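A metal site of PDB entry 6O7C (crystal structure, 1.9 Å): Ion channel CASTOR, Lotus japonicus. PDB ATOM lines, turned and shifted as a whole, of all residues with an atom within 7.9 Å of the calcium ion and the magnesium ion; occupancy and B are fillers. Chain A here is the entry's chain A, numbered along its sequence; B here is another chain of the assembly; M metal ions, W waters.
The guanidinium group of Arg 279 sits close to the side-chain carboxylate of Asp 131 (3.1 Å).
N of Asp 131 is in hydrogen-bond range of OD2 of Asp 104 (2.9 Å).
Three residues have an atom within 4 Å of the calcium ion: Asp 131, Asp 133 and Asp 280.
The nearest printed residue that does not touch the calcium ion is Arg 279 (4.6 Å).
Gly 316 touches the magnesium ion (O to MG, 3.97 Å).
Of the 20 residues printed, 2 come within 4 Å of the magnesium ion.
Along chain A the residues within 4 Å of the magnesium ion span positions 133 to 316.
The nearest printed residue that does not touch the magnesium ion is Asp 283 (4.03 Å).
Water W6 binds the calcium ion, 2.2 Å away.
The side-chain carboxylate (OD2) of Asp 133 is bound to the calcium ion, at 2.3 Å.
The calcium ion is bound by water W3 (2.3 Å).
The side-chain carboxylate (OD2) of Asp 280 is bound to the calcium ion (2.4 Å).
The calcium ion is bound by OD2 of Asp 131 (2.4 Å).
Water W2 is bound to the calcium ion, at 2.5 Å.
The calcium ion is bound by the side-chain carboxylate (OD1) of Asp 280, 2.5 Å away.
The calcium ion is bound by OD1 of Asp 131 (2.5 Å).
The calcium ion has eight donor atoms within binding distance.
The magnesium ion is bound by water W1, water W4, water W5 and OD1 of Asp 133.
The magnesium ion has four donor atoms within binding distance.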
ATOM      1  N   ALA A 100     -14.338 -12.593 -23.314  1.00  0.00           N
ATOM      2  CA  ALA A 100     -14.125 -11.607 -22.271  1.00  0.00           C
ATOM      3  C   ALA A 100     -12.934 -10.691 -22.601  1.00  0.00           C
ATOM      4  O   ALA A 100     -12.972  -9.495 -22.330  1.00  0.00           O
ATOM      5  CB  ALA A 100     -13.890 -12.301 -20.915  1.00  0.00           C
ATOM      6  N   ASP A 101     -11.846 -11.243 -23.126  1.00  0.00           N
ATOM      7  CA  ASP A 101     -10.695 -10.365 -23.383  1.00  0.00           C
ATOM      8  C   ASP A 101     -11.008  -9.355 -24.467  1.00  0.00           C
ATOM      9  O   ASP A 101     -10.572  -8.193 -24.385  1.00  0.00           O
ATOM     10  CB  ASP A 101      -9.437 -11.161 -23.786  1.00  0.00           C
ATOM     11  CG  ASP A 101      -8.705 -11.769 -22.573  1.00  0.00           C
ATOM     12  OD1 ASP A 101      -8.960 -11.379 -21.357  1.00  0.00           O
ATOM     13  OD2 ASP A 101      -7.791 -12.592 -22.842  1.00  0.00           O
ATOM     14  N   ASP A 104     -13.126  -6.683 -22.897  1.00  0.00           N
ATOM     15  CA  ASP A 104     -12.338  -5.774 -22.043  1.00  0.00           C
ATOM     16  C   ASP A 104     -11.365  -4.897 -22.818  1.00  0.00           C
ATOM     17  O   ASP A 104     -11.077  -3.743 -22.363  1.00  0.00           O
ATOM     18  CB  ASP A 104     -11.605  -6.569 -20.982  1.00  0.00           C
ATOM     19  CG  ASP A 104     -12.565  -7.109 -19.892  1.00  0.00           C
ATOM     20  OD1 ASP A 104     -13.740  -6.617 -19.720  1.00  0.00           O
ATOM     21  OD2 ASP A 104     -12.141  -8.010 -19.147  1.00  0.00           O
ATOM     22  N   SER A 130     -15.347  -7.840 -17.947  1.00  0.00           N
ATOM     23  CA  SER A 130     -15.632  -9.265 -18.065  1.00  0.00           C
ATOM     24  C   SER A 130     -14.588 -10.152 -17.370  1.00  0.00           C
ATOM     25  O   SER A 130     -14.840 -11.343 -17.126  1.00  0.00           O
ATOM     26  CB  SER A 130     -15.655  -9.602 -19.569  1.00  0.00           C
ATOM     27  OG  SER A 130     -16.791  -8.935 -20.148  1.00  0.00           O
ATOM     28  N   ASP A 131     -13.403  -9.622 -17.090  1.00  0.00           N
ATOM     29  CA  ASP A 131     -12.342 -10.463 -16.520  1.00  0.00           C
ATOM     30  C   ASP A 131     -11.619  -9.641 -15.489  1.00  0.00           C
ATOM     31  O   ASP A 131     -11.163  -8.537 -15.795  1.00  0.00           O
ATOM     32  CB  ASP A 131     -11.449 -10.984 -17.608  1.00  0.00           C
ATOM     33  CG  ASP A 131     -10.358 -11.986 -17.114  1.00  0.00           C
ATOM     34  OD1 ASP A 131      -9.617 -11.705 -16.166  1.00  0.00           O
ATOM     35  OD2 ASP A 131     -10.344 -13.127 -17.634  1.00  0.00           O
ATOM     36  N   LEU A 132     -11.443 -10.218 -14.296  1.00  0.00           N
ATOM     37  CA  LEU A 132     -10.831  -9.468 -13.192  1.00  0.00           C
ATOM     38  C   LEU A 132      -9.415  -9.040 -13.531  1.00  0.00           C
ATOM     39  O   LEU A 132      -8.956  -7.961 -13.117  1.00  0.00           O
ATOM     40  CB  LEU A 132     -10.843 -10.372 -11.949  1.00  0.00           C
ATOM     41  CG  LEU A 132     -10.346  -9.712 -10.645  1.00  0.00           C
ATOM     42  CD1 LEU A 132     -11.314  -8.588 -10.273  1.00  0.00           C
ATOM     43  CD2 LEU A 132     -10.374 -10.823  -9.536  1.00  0.00           C
ATOM     44  N   ASP A 133      -8.688  -9.855 -14.261  1.00  0.00           N
ATOM     45  CA  ASP A 133      -7.282  -9.535 -14.544  1.00  0.00           C
ATOM     46  C   ASP A 133      -7.132  -8.298 -15.417  1.00  0.00           C
ATOM     47  O   ASP A 133      -6.039  -7.733 -15.521  1.00  0.00           O
ATOM     48  CB  ASP A 133      -6.711 -10.772 -15.235  1.00  0.00           C
ATOM     49  CG  ASP A 133      -6.675 -12.000 -14.278  1.00  0.00           C
ATOM     50  OD1 ASP A 133      -6.057 -11.822 -13.220  1.00  0.00           O
ATOM     51  OD2 ASP A 133      -7.266 -13.040 -14.596  1.00  0.00           O
ATOM     52  N   ASN A 134      -8.204  -7.881 -16.075  1.00  0.00           N
ATOM     53  CA  ASN A 134      -8.167  -6.686 -16.896  1.00  0.00           C
ATOM     54  C   ASN A 134      -8.586  -5.417 -16.156  1.00  0.00           C
ATOM     55  O   ASN A 134      -8.431  -4.323 -16.699  1.00  0.00           O
ATOM     56  CB  ASN A 134      -9.066  -6.934 -18.102  1.00  0.00           C
ATOM     57  CG  ASN A 134      -8.566  -8.086 -18.942  1.00  0.00           C
ATOM     58  OD1 ASN A 134      -7.324  -8.261 -19.096  1.00  0.00           O
ATOM     59  ND2 ASN A 134      -9.457  -8.810 -19.537  1.00  0.00           N
ATOM     60  N   HIS A 152     -18.331 -11.104 -14.256  1.00  0.00           N
ATOM     61  CA  HIS A 152     -18.011 -12.501 -14.043  1.00  0.00           C
ATOM     62  C   HIS A 152     -17.706 -12.728 -12.566  1.00  0.00           C
ATOM     63  O   HIS A 152     -18.084 -13.756 -11.992  1.00  0.00           O
ATOM     64  CB  HIS A 152     -16.781 -12.813 -14.908  1.00  0.00           C
ATOM     65  CG  HIS A 152     -16.404 -14.254 -14.988  1.00  0.00           C
ATOM     66  ND1 HIS A 152     -17.238 -15.222 -15.540  1.00  0.00           N
ATOM     67  CD2 HIS A 152     -15.286 -14.899 -14.572  1.00  0.00           C
ATOM     68  CE1 HIS A 152     -16.605 -16.390 -15.541  1.00  0.00           C
ATOM     69  NE2 HIS A 152     -15.414 -16.215 -14.975  1.00  0.00           N
ATOM     70  N   ARG A 279     -13.883 -19.992 -16.114  1.00  0.00           N
ATOM     71  CA  ARG A 279     -12.759 -19.089 -16.284  1.00  0.00           C
ATOM     72  C   ARG A 279     -12.429 -18.409 -14.963  1.00  0.00           C
ATOM     73  O   ARG A 279     -13.322 -17.946 -14.233  1.00  0.00           O
ATOM     74  CB  ARG A 279     -13.092 -18.003 -17.332  1.00  0.00           C
ATOM     75  CG  ARG A 279     -11.999 -16.909 -17.398  1.00  0.00           C
ATOM     76  CD  ARG A 279     -12.144 -16.100 -18.692  1.00  0.00           C
ATOM     77  NE  ARG A 279     -13.513 -15.630 -18.869  1.00  0.00           N
ATOM     78  CZ  ARG A 279     -14.065 -14.581 -18.256  1.00  0.00           C
ATOM     79  NH1 ARG A 279     -13.335 -13.815 -17.437  1.00  0.00           N
ATOM     80  NH2 ARG A 279     -15.385 -14.299 -18.481  1.00  0.00           N
ATOM     81  N   ASP A 280     -11.159 -18.409 -14.622  1.00  0.00           N
ATOM     82  CA  ASP A 280     -10.701 -17.709 -13.390  1.00  0.00           C
ATOM     83  C   ASP A 280     -11.288 -18.378 -12.138  1.00  0.00           C
ATOM     84  O   ASP A 280     -11.478 -17.741 -11.103  1.00  0.00           O
ATOM     85  CB  ASP A 280     -11.006 -16.183 -13.349  1.00  0.00           C
ATOM     86  CG  ASP A 280     -10.102 -15.347 -14.344  1.00  0.00           C
ATOM     87  OD1 ASP A 280      -9.104 -15.944 -14.782  1.00  0.00           O
ATOM     88  OD2 ASP A 280     -10.393 -14.178 -14.722  1.00  0.00           O
ATOM     89  N   MET A 281     -11.470 -19.696 -12.177  1.00  0.00           N
ATOM     90  CA  MET A 281     -12.155 -20.382 -11.083  1.00  0.00           C
ATOM     91  C   MET A 281     -11.353 -20.330  -9.790  1.00  0.00           C
ATOM     92  O   MET A 281     -11.924 -20.443  -8.685  1.00  0.00           O
ATOM     93  CB  MET A 281     -12.408 -21.839 -11.459  1.00  0.00           C
ATOM     94  CG  MET A 281     -13.407 -22.527 -10.442  1.00  0.00           C
ATOM     95  SD  MET A 281     -14.013 -24.058 -11.112  1.00  0.00           S
ATOM     96  CE  MET A 281     -12.572 -25.119 -11.192  1.00  0.00           C
ATOM     97  N   GLU A 282     -10.037 -20.077  -9.895  1.00  0.00           N
ATOM     98  CA  GLU A 282      -9.271 -19.891  -8.669  1.00  0.00           C
ATOM     99  C   GLU A 282      -9.793 -18.730  -7.856  1.00  0.00           C
ATOM    100  O   GLU A 282      -9.588 -18.694  -6.629  1.00  0.00           O
ATOM    101  CB  GLU A 282      -7.788 -19.682  -9.011  1.00  0.00           C
ATOM    102  CG  GLU A 282      -7.564 -18.460  -9.925  1.00  0.00           C
ATOM    103  CD  GLU A 282      -7.706 -18.781 -11.444  1.00  0.00           C
ATOM    104  OE1 GLU A 282      -8.206 -19.852 -11.831  1.00  0.00           O
ATOM    105  OE2 GLU A 282      -7.256 -17.956 -12.259  1.00  0.00           O
ATOM    106  N   ASP A 283     -10.402 -17.728  -8.491  1.00  0.00           N
ATOM    107  CA  ASP A 283     -10.947 -16.605  -7.733  1.00  0.00           C
ATOM    108  C   ASP A 283     -12.137 -17.081  -6.861  1.00  0.00           C
ATOM    109  O   ASP A 283     -12.325 -16.622  -5.707  1.00  0.00           O
ATOM    110  CB  ASP A 283     -11.395 -15.501  -8.697  1.00  0.00           C
ATOM    111  CG  ASP A 283     -10.183 -14.886  -9.488  1.00  0.00           C
ATOM    112  OD1 ASP A 283      -9.073 -15.062  -8.951  1.00  0.00           O
ATOM    113  OD2 ASP A 283     -10.414 -14.254 -10.548  1.00  0.00           O
ATOM    114  N   ASP A 315      -0.965 -20.579 -11.782  1.00  0.00           N
ATOM    115  CA  ASP A 315      -0.815 -19.413 -12.678  1.00  0.00           C
ATOM    116  C   ASP A 315      -1.856 -18.339 -12.432  1.00  0.00           C
ATOM    117  O   ASP A 315      -1.604 -17.168 -12.761  1.00  0.00           O
ATOM    118  CB  ASP A 315      -0.892 -19.816 -14.162  1.00  0.00           C
ATOM    119  CG  ASP A 315       0.294 -20.631 -14.638  1.00  0.00           C
ATOM    120  OD1 ASP A 315       1.382 -20.682 -14.001  1.00  0.00           O
ATOM    121  OD2 ASP A 315       0.159 -21.175 -15.744  1.00  0.00           O
ATOM    122  N   GLY A 316      -3.063 -18.699 -11.918  1.00  0.00           N
ATOM    123  CA  GLY A 316      -4.002 -17.646 -11.562  1.00  0.00           C
ATOM    124  C   GLY A 316      -3.802 -17.093 -10.186  1.00  0.00           C
ATOM    125  O   GLY A 316      -4.641 -16.364  -9.662  1.00  0.00           O
ATOM    126  N   GLY A 317      -2.691 -17.449  -9.556  1.00  0.00           N
ATOM    127  CA  GLY A 317      -2.363 -16.881  -8.277  1.00  0.00           C
ATOM    128  C   GLY A 317      -2.824 -17.634  -7.062  1.00  0.00           C
ATOM    129  O   GLY A 317      -2.675 -17.092  -5.958  1.00  0.00           O
ATOM    130  N   LEU A 318      -3.360 -18.855  -7.195  1.00  0.00           N
ATOM    131  CA  LEU A 318      -3.815 -19.609  -6.018  1.00  0.00           C
ATOM    132  C   LEU A 318      -2.736 -20.592  -5.548  1.00  0.00           C
ATOM    133  O   LEU A 318      -2.350 -21.491  -6.302  1.00  0.00           O
ATOM    134  CB  LEU A 318      -5.103 -20.374  -6.320  1.00  0.00           C
ATOM    135  CG  LEU A 318      -5.625 -21.205  -5.174  1.00  0.00           C
ATOM    136  CD1 LEU A 318      -5.985 -20.274  -4.021  1.00  0.00           C
ATOM    137  CD2 LEU A 318      -6.812 -21.940  -5.605  1.00  0.00           C
ATOM    138  N   GLU A 358     -15.237 -22.649 -19.055  1.00  0.00           N
ATOM    139  CA  GLU A 358     -14.489 -21.696 -19.880  1.00  0.00           C
ATOM    140  C   GLU A 358     -14.414 -22.138 -21.339  1.00  0.00           C
ATOM    141  O   GLU A 358     -14.194 -21.296 -22.223  1.00  0.00           O
ATOM    142  CB  GLU A 358     -13.077 -21.452 -19.332  1.00  0.00           C
ATOM    143  CG  GLU A 358     -12.248 -22.676 -19.228  1.00  0.00           C
ATOM    144  CD  GLU A 358     -10.819 -22.320 -18.765  1.00  0.00           C
ATOM    145  OE1 GLU A 358     -10.573 -21.122 -18.448  1.00  0.00           O
ATOM    146  OE2 GLU A 358      -9.940 -23.224 -18.842  1.00  0.00           O
ATOM    147  N   ILE B 337       1.357 -13.805 -17.725  1.00  0.00           N
ATOM    148  CA  ILE B 337       1.152 -14.514 -16.451  1.00  0.00           C
ATOM    149  C   ILE B 337       2.158 -13.986 -15.434  1.00  0.00           C
ATOM    150  O   ILE B 337       3.373 -14.139 -15.611  1.00  0.00           O
ATOM    151  CB  ILE B 337       1.302 -16.037 -16.578  1.00  0.00           C
ATOM    152  CG1 ILE B 337       0.251 -16.626 -17.556  1.00  0.00           C
ATOM    153  CG2 ILE B 337       1.246 -16.671 -15.200  1.00  0.00           C
ATOM    154  CD1 ILE B 337      -1.146 -16.155 -17.278  1.00  0.00           C
HETATM  155 CA    CA M   1      -8.575 -14.015 -16.259  1.00  0.00          CA
HETATM  156 MG    MG M   2      -6.472 -13.390 -11.540  1.00  0.00          MG
HETATM  157  O   HOH W   1      -6.645 -11.810 -10.485  1.00  0.00           O
HETATM  158  O   HOH W   2      -6.492 -15.363 -16.110  1.00  0.00           O
HETATM  159  O   HOH W   3      -7.167 -13.157 -17.928  1.00  0.00           O
HETATM  160  O   HOH W   4      -4.444 -13.635 -11.538  1.00  0.00           O
HETATM  161  O   HOH W   5      -6.323 -15.062 -12.850  1.00  0.00           O
HETATM  162  O   HOH W   6      -8.782 -15.626 -17.722  1.00  0.00           O
